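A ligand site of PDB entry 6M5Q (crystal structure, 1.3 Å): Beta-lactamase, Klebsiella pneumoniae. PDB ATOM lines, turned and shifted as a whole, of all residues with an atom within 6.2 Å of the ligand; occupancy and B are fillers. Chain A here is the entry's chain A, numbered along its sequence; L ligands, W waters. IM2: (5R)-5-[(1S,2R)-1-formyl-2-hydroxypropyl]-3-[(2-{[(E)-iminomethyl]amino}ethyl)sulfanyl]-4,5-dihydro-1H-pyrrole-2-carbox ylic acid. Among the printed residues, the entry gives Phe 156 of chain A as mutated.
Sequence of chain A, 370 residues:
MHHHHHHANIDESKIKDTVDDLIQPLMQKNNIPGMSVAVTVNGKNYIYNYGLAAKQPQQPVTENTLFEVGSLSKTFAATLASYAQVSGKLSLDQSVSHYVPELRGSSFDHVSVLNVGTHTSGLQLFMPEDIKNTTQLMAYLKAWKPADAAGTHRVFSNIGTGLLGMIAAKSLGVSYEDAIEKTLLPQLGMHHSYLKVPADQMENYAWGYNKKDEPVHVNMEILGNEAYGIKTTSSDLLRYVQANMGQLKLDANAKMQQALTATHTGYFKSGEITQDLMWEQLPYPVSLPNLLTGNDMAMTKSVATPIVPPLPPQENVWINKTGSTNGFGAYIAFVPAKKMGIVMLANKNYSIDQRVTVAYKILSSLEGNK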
ATOM      1  N   VAL A  69      16.486  -8.865  13.181  1.00  0.00           N
ATOM      2  CA  VAL A  69      16.301  -9.592  11.929  1.00  0.00           C
ATOM      3  C   VAL A  69      15.836 -11.020  12.123  1.00  0.00           C
ATOM      4  O   VAL A  69      15.661 -11.744  11.138  1.00  0.00           O
ATOM      5  CB  VAL A  69      17.533  -9.523  11.015  1.00  0.00           C
ATOM      6  CG1 VAL A  69      17.837  -8.049  10.699  1.00  0.00           C
ATOM      7  CG2 VAL A  69      18.734 -10.241  11.646  1.00  0.00           C
ATOM      8  N   GLY A  70      15.582 -11.433  13.354  1.00  0.00           N
ATOM      9  CA  GLY A  70      14.963 -12.725  13.559  1.00  0.00           C
ATOM     10  C   GLY A  70      15.752 -13.837  12.911  1.00  0.00           C
ATOM     11  O   GLY A  70      16.979 -13.922  13.055  1.00  0.00           O
ATOM     12  N   SER A  71      15.047 -14.700  12.162  1.00  0.00           N
ATOM     13  CA  SER A  71      15.678 -15.879  11.579  1.00  0.00           C
ATOM     14  C   SER A  71      16.728 -15.582  10.522  1.00  0.00           C
ATOM     15  O   SER A  71      17.443 -16.520  10.135  1.00  0.00           O
ATOM     16  CB  SER A  71      14.638 -16.852  11.033  1.00  0.00           C
ATOM     17  OG  SER A  71      13.784 -17.322  12.080  1.00  0.00           O
ATOM     18  N   LEU A  72      16.913 -14.329  10.090  1.00  0.00           N
ATOM     19  CA  LEU A  72      18.132 -14.079   9.318  1.00  0.00           C
ATOM     20  C   LEU A  72      19.369 -14.428  10.128  1.00  0.00           C
ATOM     21  O   LEU A  72      20.428 -14.708   9.557  1.00  0.00           O
ATOM     22  CB  LEU A  72      18.248 -12.616   8.884  1.00  0.00           C
ATOM     23  CG  LEU A  72      17.293 -12.037   7.843  1.00  0.00           C
ATOM     24  CD1 LEU A  72      17.778 -10.684   7.349  1.00  0.00           C
ATOM     25  CD2 LEU A  72      17.194 -12.966   6.737  1.00  0.00           C
ATOM     26  N   LYS A  74      20.000 -17.032  11.555  1.00  0.00           N
ATOM     27  CA  LYS A  74      20.400 -18.406  11.311  1.00  0.00           C
ATOM     28  C   LYS A  74      21.482 -18.498  10.233  1.00  0.00           C
ATOM     29  O   LYS A  74      22.287 -19.434  10.247  1.00  0.00           O
ATOM     30  CB  LYS A  74      19.202 -19.260  10.899  1.00  0.00           C
ATOM     31  CG  LYS A  74      18.098 -19.265  11.962  1.00  0.00           C
ATOM     32  CD  LYS A  74      16.961 -20.210  11.617  1.00  0.00           C
ATOM     33  CE  LYS A  74      16.011 -20.269  12.821  1.00  0.00           C
ATOM     34  NZ  LYS A  74      14.979 -21.335  12.666  1.00  0.00           N
ATOM     35  N   HIS A 119      17.725 -27.948   8.489  1.00  0.00           N
ATOM     36  CA  HIS A 119      16.361 -28.134   8.991  1.00  0.00           C
ATOM     37  C   HIS A 119      15.839 -29.534   8.732  1.00  0.00           C
ATOM     38  O   HIS A 119      14.634 -29.726   8.574  1.00  0.00           O
ATOM     39  CB  HIS A 119      15.397 -27.057   8.486  1.00  0.00           C
ATOM     40  CG  HIS A 119      15.793 -25.669   8.904  1.00  0.00           C
ATOM     41  ND1 HIS A 119      16.103 -25.360  10.210  1.00  0.00           N
ATOM     42  CD2 HIS A 119      15.937 -24.526   8.193  1.00  0.00           C
ATOM     43  CE1 HIS A 119      16.407 -24.067  10.286  1.00  0.00           C
ATOM     44  NE2 HIS A 119      16.311 -23.541   9.077  1.00  0.00           N
ATOM     45  N   LEU A 125      10.158 -26.431  15.871  1.00  0.00           N
ATOM     46  CA  LEU A 125      10.527 -25.040  15.633  1.00  0.00           C
ATOM     47  C   LEU A 125      11.010 -24.352  16.894  1.00  0.00           C
ATOM     48  O   LEU A 125      12.093 -23.741  16.904  1.00  0.00           O
ATOM     49  CB  LEU A 125       9.339 -24.291  15.012  1.00  0.00           C
ATOM     50  CG  LEU A 125       9.565 -22.790  14.771  1.00  0.00           C
ATOM     51  CD1 LEU A 125      10.814 -22.525  13.912  1.00  0.00           C
ATOM     52  CD2 LEU A 125       8.319 -22.215  14.078  1.00  0.00           C
ATOM     53  N   PHE A 126      10.241 -24.425  17.972  1.00  0.00           N
ATOM     54  CA  PHE A 126      10.484 -23.586  19.139  1.00  0.00           C
ATOM     55  C   PHE A 126      11.084 -24.356  20.292  1.00  0.00           C
ATOM     56  O   PHE A 126      10.635 -25.461  20.633  1.00  0.00           O
ATOM     57  CB  PHE A 126       9.192 -22.894  19.602  1.00  0.00           C
ATOM     58  CG  PHE A 126       8.695 -21.850  18.643  1.00  0.00           C
ATOM     59  CD1 PHE A 126       9.410 -20.691  18.430  1.00  0.00           C
ATOM     60  CD2 PHE A 126       7.520 -22.039  17.961  1.00  0.00           C
ATOM     61  CE1 PHE A 126       8.957 -19.727  17.547  1.00  0.00           C
ATOM     62  CE2 PHE A 126       7.040 -21.080  17.063  1.00  0.00           C
ATOM     63  CZ  PHE A 126       7.779 -19.916  16.847  1.00  0.00           C
ATOM     64  N   PHE A 156      11.512 -26.407   9.867  1.00  0.00           N
ATOM     65  CA  PHE A 156      12.308 -25.276  10.326  1.00  0.00           C
ATOM     66  C   PHE A 156      12.434 -25.351  11.831  1.00  0.00           C
ATOM     67  O   PHE A 156      11.448 -25.600  12.528  1.00  0.00           O
ATOM     68  CB  PHE A 156      11.645 -23.966   9.909  1.00  0.00           C
ATOM     69  CG  PHE A 156      11.644 -23.761   8.425  1.00  0.00           C
ATOM     70  CD1 PHE A 156      12.760 -23.259   7.789  1.00  0.00           C
ATOM     71  CD2 PHE A 156      10.535 -24.116   7.670  1.00  0.00           C
ATOM     72  CE1 PHE A 156      12.768 -23.091   6.409  1.00  0.00           C
ATOM     73  CE2 PHE A 156      10.531 -23.943   6.292  1.00  0.00           C
ATOM     74  CZ  PHE A 156      11.657 -23.432   5.654  1.00  0.00           C
ATOM     75  N   SER A 157      13.649 -25.150  12.343  1.00  0.00           N
ATOM     76  CA  SER A 157      13.903 -25.400  13.749  1.00  0.00           C
ATOM     77  C   SER A 157      14.832 -24.363  14.357  1.00  0.00           C
ATOM     78  O   SER A 157      15.973 -24.228  13.906  1.00  0.00           O
ATOM     79  CB  SER A 157      14.473 -26.802  13.958  1.00  0.00           C
ATOM     80  OG  SER A 157      14.710 -27.026  15.342  1.00  0.00           O
ATOM     81  N   ASN A 158      14.387 -23.685  15.412  1.00  0.00           N
ATOM     82  CA  ASN A 158      15.316 -22.860  16.179  1.00  0.00           C
ATOM     83  C   ASN A 158      16.259 -23.725  17.007  1.00  0.00           C
ATOM     84  O   ASN A 158      17.418 -23.341  17.212  1.00  0.00           O
ATOM     85  CB  ASN A 158      14.579 -21.910  17.113  1.00  0.00           C
ATOM     86  CG  ASN A 158      13.751 -20.882  16.360  1.00  0.00           C
ATOM     87  OD1 ASN A 158      13.935 -20.656  15.153  1.00  0.00           O
ATOM     88  ND2 ASN A 158      12.872 -20.205  17.089  1.00  0.00           N
ATOM     89  N   THR A 161      19.083 -24.984  14.732  1.00  0.00           N
ATOM     90  CA  THR A 161      20.053 -23.927  14.435  1.00  0.00           C
ATOM     91  C   THR A 161      20.909 -23.644  15.660  1.00  0.00           C
ATOM     92  O   THR A 161      22.122 -23.366  15.554  1.00  0.00           O
ATOM     93  CB  THR A 161      19.355 -22.644  14.006  1.00  0.00           C
ATOM     94  OG1 THR A 161      18.417 -22.933  12.963  1.00  0.00           O
ATOM     95  CG2 THR A 161      20.399 -21.654  13.454  1.00  0.00           C
ATOM     96  N   ALA A 227      19.481 -18.479  16.684  1.00  0.00           N
ATOM     97  CA  ALA A 227      18.256 -18.531  15.898  1.00  0.00           C
ATOM     98  C   ALA A 227      17.672 -17.144  15.632  1.00  0.00           C
ATOM     99  O   ALA A 227      17.037 -16.945  14.587  1.00  0.00           O
ATOM    100  CB  ALA A 227      17.209 -19.417  16.596  1.00  0.00           C
ATOM    101  N   TYR A 228      17.863 -16.179  16.550  1.00  0.00           N
ATOM    102  CA  TYR A 228      17.182 -14.900  16.399  1.00  0.00           C
ATOM    103  C   TYR A 228      17.913 -13.751  17.089  1.00  0.00           C
ATOM    104  O   TYR A 228      17.279 -12.723  17.352  1.00  0.00           O
ATOM    105  CB  TYR A 228      15.691 -14.994  16.896  1.00  0.00           C
ATOM    106  CG  TYR A 228      15.547 -15.498  18.321  1.00  0.00           C
ATOM    107  CD1 TYR A 228      15.687 -14.640  19.416  1.00  0.00           C
ATOM    108  CD2 TYR A 228      15.306 -16.836  18.581  1.00  0.00           C
ATOM    109  CE1 TYR A 228      15.583 -15.112  20.730  1.00  0.00           C
ATOM    110  CE2 TYR A 228      15.204 -17.322  19.894  1.00  0.00           C
ATOM    111  CZ  TYR A 228      15.352 -16.448  20.947  1.00  0.00           C
ATOM    112  OH  TYR A 228      15.253 -16.883  22.260  1.00  0.00           O
ATOM    113  N   MET A 278      21.196 -23.157   5.756  1.00  0.00           N
ATOM    114  CA  MET A 278      20.239 -22.136   6.207  1.00  0.00           C
ATOM    115  C   MET A 278      19.648 -21.272   5.094  1.00  0.00           C
ATOM    116  O   MET A 278      18.422 -21.118   5.036  1.00  0.00           O
ATOM    117  CB  MET A 278      20.800 -21.273   7.368  1.00  0.00           C
ATOM    118  CG  MET A 278      20.981 -22.088   8.665  1.00  0.00           C
ATOM    119  SD  MET A 278      19.382 -22.651   9.309  1.00  0.00           S
ATOM    120  CE  MET A 278      19.916 -24.063  10.277  1.00  0.00           C
ATOM    121  N   GLU A 280      18.021 -20.410   1.525  1.00  0.00           N
ATOM    122  CA  GLU A 280      17.140 -21.122   0.604  1.00  0.00           C
ATOM    123  C   GLU A 280      17.308 -20.506  -0.773  1.00  0.00           C
ATOM    124  O   GLU A 280      17.577 -19.303  -0.884  1.00  0.00           O
ATOM    125  CB  GLU A 280      15.649 -20.919   1.000  1.00  0.00           C
ATOM    126  CG  GLU A 280      15.318 -21.385   2.401  1.00  0.00           C
ATOM    127  CD  GLU A 280      13.829 -21.294   2.674  1.00  0.00           C
ATOM    128  OE1 GLU A 280      13.053 -20.872   1.784  1.00  0.00           O
ATOM    129  OE2 GLU A 280      13.442 -21.635   3.808  1.00  0.00           O
ATOM    130  N   GLY A 294       6.686 -20.951  -2.626  1.00  0.00           N
ATOM    131  CA  GLY A 294       7.775 -21.429  -1.793  1.00  0.00           C
ATOM    132  C   GLY A 294       7.651 -21.038  -0.335  1.00  0.00           C
ATOM    133  O   GLY A 294       8.320 -21.637   0.514  1.00  0.00           O
ATOM    134  N   ASN A 295       6.824 -20.048  -0.013  1.00  0.00           N
ATOM    135  CA  ASN A 295       6.672 -19.595   1.367  1.00  0.00           C
ATOM    136  C   ASN A 295       5.324 -20.010   1.961  1.00  0.00           C
ATOM    137  O   ASN A 295       4.721 -20.998   1.543  1.00  0.00           O
ATOM    138  CB  ASN A 295       6.846 -18.083   1.466  1.00  0.00           C
ATOM    139  CG  ASN A 295       8.105 -17.596   0.756  1.00  0.00           C
ATOM    140  OD1 ASN A 295       8.037 -16.967  -0.300  1.00  0.00           O
ATOM    141  ND2 ASN A 295       9.265 -17.861   1.356  1.00  0.00           N
ATOM    142  N   ASN A 320      17.830 -16.488  -0.827  1.00  0.00           N
ATOM    143  CA  ASN A 320      17.051 -15.579   0.025  1.00  0.00           C
ATOM    144  C   ASN A 320      16.858 -16.164   1.417  1.00  0.00           C
ATOM    145  O   ASN A 320      17.075 -17.359   1.666  1.00  0.00           O
ATOM    146  CB  ASN A 320      15.726 -15.127  -0.650  1.00  0.00           C
ATOM    147  CG  ASN A 320      14.664 -16.236  -0.754  1.00  0.00           C
ATOM    148  OD1 ASN A 320      14.912 -17.447  -0.515  1.00  0.00           O
ATOM    149  ND2 ASN A 320      13.478 -15.837  -1.128  1.00  0.00           N
ATOM    150  N   LYS A 321      16.434 -15.277   2.316  1.00  0.00           N
ATOM    151  CA  LYS A 321      16.093 -15.686   3.671  1.00  0.00           C
ATOM    152  C   LYS A 321      15.162 -14.628   4.259  1.00  0.00           C
ATOM    153  O   LYS A 321      15.442 -13.437   4.152  1.00  0.00           O
ATOM    154  CB  LYS A 321      17.364 -15.793   4.533  1.00  0.00           C
ATOM    155  CG  LYS A 321      17.115 -16.309   5.945  1.00  0.00           C
ATOM    156  CD  LYS A 321      16.981 -17.801   5.915  1.00  0.00           C
ATOM    157  CE  LYS A 321      16.366 -18.296   7.212  1.00  0.00           C
ATOM    158  NZ  LYS A 321      14.904 -18.165   7.201  1.00  0.00           N
ATOM    159  N   THR A 322      14.078 -15.080   4.884  1.00  0.00           N
ATOM    160  CA  THR A 322      13.196 -14.218   5.664  1.00  0.00           C
ATOM    161  C   THR A 322      13.542 -14.366   7.143  1.00  0.00           C
ATOM    162  O   THR A 322      14.088 -15.375   7.575  1.00  0.00           O
ATOM    163  CB  THR A 322      11.719 -14.611   5.484  1.00  0.00           C
ATOM    164  OG1 THR A 322      11.521 -15.939   5.964  1.00  0.00           O
ATOM    165  CG2 THR A 322      11.321 -14.552   4.025  1.00  0.00           C
ATOM    166  N   GLY A 323      13.212 -13.351   7.904  1.00  0.00           N
ATOM    167  CA  GLY A 323      13.319 -13.456   9.348  1.00  0.00           C
ATOM    168  C   GLY A 323      12.345 -12.530  10.019  1.00  0.00           C
ATOM    169  O   GLY A 323      12.056 -11.436   9.525  1.00  0.00           O
ATOM    170  N   SER A 324      11.857 -12.955  11.180  1.00  0.00           N
ATOM    171  CA  SER A 324      10.901 -12.135  11.919  1.00  0.00           C
ATOM    172  C   SER A 324      11.100 -12.317  13.408  1.00  0.00           C
ATOM    173  O   SER A 324      11.571 -13.355  13.863  1.00  0.00           O
ATOM    174  CB  SER A 324       9.455 -12.504  11.582  1.00  0.00           C
ATOM    175  OG  SER A 324       9.233 -12.543  10.168  1.00  0.00           O
ATOM    176  N   THR A 325      10.694 -11.302  14.163  1.00  0.00           N
ATOM    177  CA  THR A 325      10.447 -11.436  15.596  1.00  0.00           C
ATOM    178  C   THR A 325       9.043 -10.883  15.837  1.00  0.00           C
ATOM    179  O   THR A 325       8.341 -10.489  14.900  1.00  0.00           O
ATOM    180  CB  THR A 325      11.480 -10.666  16.424  1.00  0.00           C
ATOM    181  OG1 THR A 325      11.356  -9.286  16.108  1.00  0.00           O
ATOM    182  CG2 THR A 325      12.929 -11.197  16.176  1.00  0.00           C
ATOM    183  N   ILE A 352       5.085 -12.387   4.661  1.00  0.00           N
ATOM    184  CA  ILE A 352       6.221 -12.740   3.811  1.00  0.00           C
ATOM    185  C   ILE A 352       5.896 -12.574   2.329  1.00  0.00           C
ATOM    186  O   ILE A 352       6.773 -12.171   1.548  1.00  0.00           O
ATOM    187  CB  ILE A 352       6.718 -14.152   4.165  1.00  0.00           C
ATOM    188  CG1 ILE A 352       7.502 -14.107   5.478  1.00  0.00           C
ATOM    189  CG2 ILE A 352       7.567 -14.754   3.050  1.00  0.00           C
ATOM    190  CD1 ILE A 352       7.896 -15.476   5.953  1.00  0.00           C
HETATM  191  C7  IM2 L   1      12.542 -16.828  12.180  1.00  0.00           C
HETATM  192  C2  IM2 L   1      10.719 -19.016  10.538  1.00  0.00           C
HETATM  193  C6  IM2 L   1      11.599 -17.459  13.276  1.00  0.00           C
HETATM  194  C5  IM2 L   1      11.097 -18.737  12.850  1.00  0.00           C
HETATM  195  C3  IM2 L   1      12.039 -19.599  10.934  1.00  0.00           C
HETATM  196  O7  IM2 L   1      12.210 -15.813  11.640  1.00  0.00           O
HETATM  197  C61 IM2 L   1      12.418 -17.659  14.585  1.00  0.00           C
HETATM  198  O62 IM2 L   1      11.531 -18.126  15.560  1.00  0.00           O
HETATM  199  C62 IM2 L   1      13.052 -16.349  15.008  1.00  0.00           C
HETATM  200  N4  IM2 L   1      12.236 -19.605  12.236  1.00  0.00           N
HETATM  201  C31 IM2 L   1      13.158 -19.888   9.964  1.00  0.00           C
HETATM  202  O31 IM2 L   1      13.204 -19.180   8.925  1.00  0.00           O
HETATM  203  O32 IM2 L   1      13.970 -20.814  10.204  1.00  0.00           O
HETATM  204  S21 IM2 L   1       9.805 -20.081   9.378  1.00  0.00           S
HETATM  205  C22 IM2 L   1      10.602 -20.314   7.732  1.00  0.00           C
HETATM  206  C23 IM2 L   1      10.914 -19.078   6.861  1.00  0.00           C
HETATM  207  N24 IM2 L   1      11.113 -19.449   5.450  1.00  0.00           N
HETATM  208  C25 IM2 L   1      12.122 -18.996   4.462  1.00  0.00           C
HETATM  209  N26 IM2 L   1      13.093 -18.163   4.570  1.00  0.00           N
HETATM  210  C1  IM2 L   1      10.041 -18.649  11.688  1.00  0.00           C
HETATM  211  O   HOH W   1      15.727 -21.037   8.368  1.00  0.00           O
HETATM  212  O   HOH W   2       7.532 -19.090   7.598  1.00  0.00           O
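N of Ser 324 is in hydrogen-bond range of O7 of the ligand (2.9 Å). The side-chain hydroxyl of Ser 71 is covalently linked to a carbon (C7) of the ligand, 1.3 Å away. N26 of the ligand lies within hydrogen-bond range of OG1 of Thr 322, 3.1 Å away. The side-chain amide nitrogen of Asn 158 lies within hydrogen-bond range of an oxygen (O62) of the ligand, at 2.9 Å. The side-chain amino group (NZ) of Lys 74 is in salt-bridge range of an oxygen (O32) of the ligand (2.7 Å). NZ of Lys 321 lies within salt-bridge range of O31 of the ligand, 2.6 Å away. OE2 of Glu 280 lies within salt-bridge range of N26 of the ligand, 3.6 Å away. O7 of the ligand lies close to N of Ser 71, 3.1 Å away.
N of Asn 158 lies within hydrogen-bond range of O of Leu 125 (2.7 Å). A ring nitrogen (ND1) of His 119 sits at hydrogen-bond distance from the backbone NH (N) of Ser 157 (3.3 Å). O of Ser 157 sits at hydrogen-bond distance from NZ of Lys 74 (3.3 Å). OD1 of Asn 158 lies within hydrogen-bond range of NZ of Lys 74 (2.8 Å). The backbone NH of Asn 320 is in hydrogen-bond range of the backbone carbonyl oxygen of Glu 280. A ring nitrogen (NE2) of His 119 lies within hydrogen-bond range of the side-chain sulfur (SD) of Met 278, at 3.2 Å.
Merely in contact with the ligand: His 119 (3.8 Å), Leu 125 (3.7 Å), Phe 126 (3.6 Å), Phe 156 (3.6 Å), Tyr 228 (3.5 Å) and Gly 323 (3.5 Å). Hydrophobic or aromatic side chains that line the ligand: Leu 125, Phe 126, Phe 156 and Tyr 228. 13 residues have an atom within 4 Å of the ligand: Ser 71, Lys 74, His 119, Leu 125, Phe 126, Phe 156, Asn 158, Tyr 228, Glu 280, Lys 321, Thr 322, Gly 323 and Ser 324.
Water W1 lies within hydrogen-bond range of O32 of the ligand (2.6 Å), NE2 of His 119 (2.7 Å) and NZ of Lys 321 (3.2 Å).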
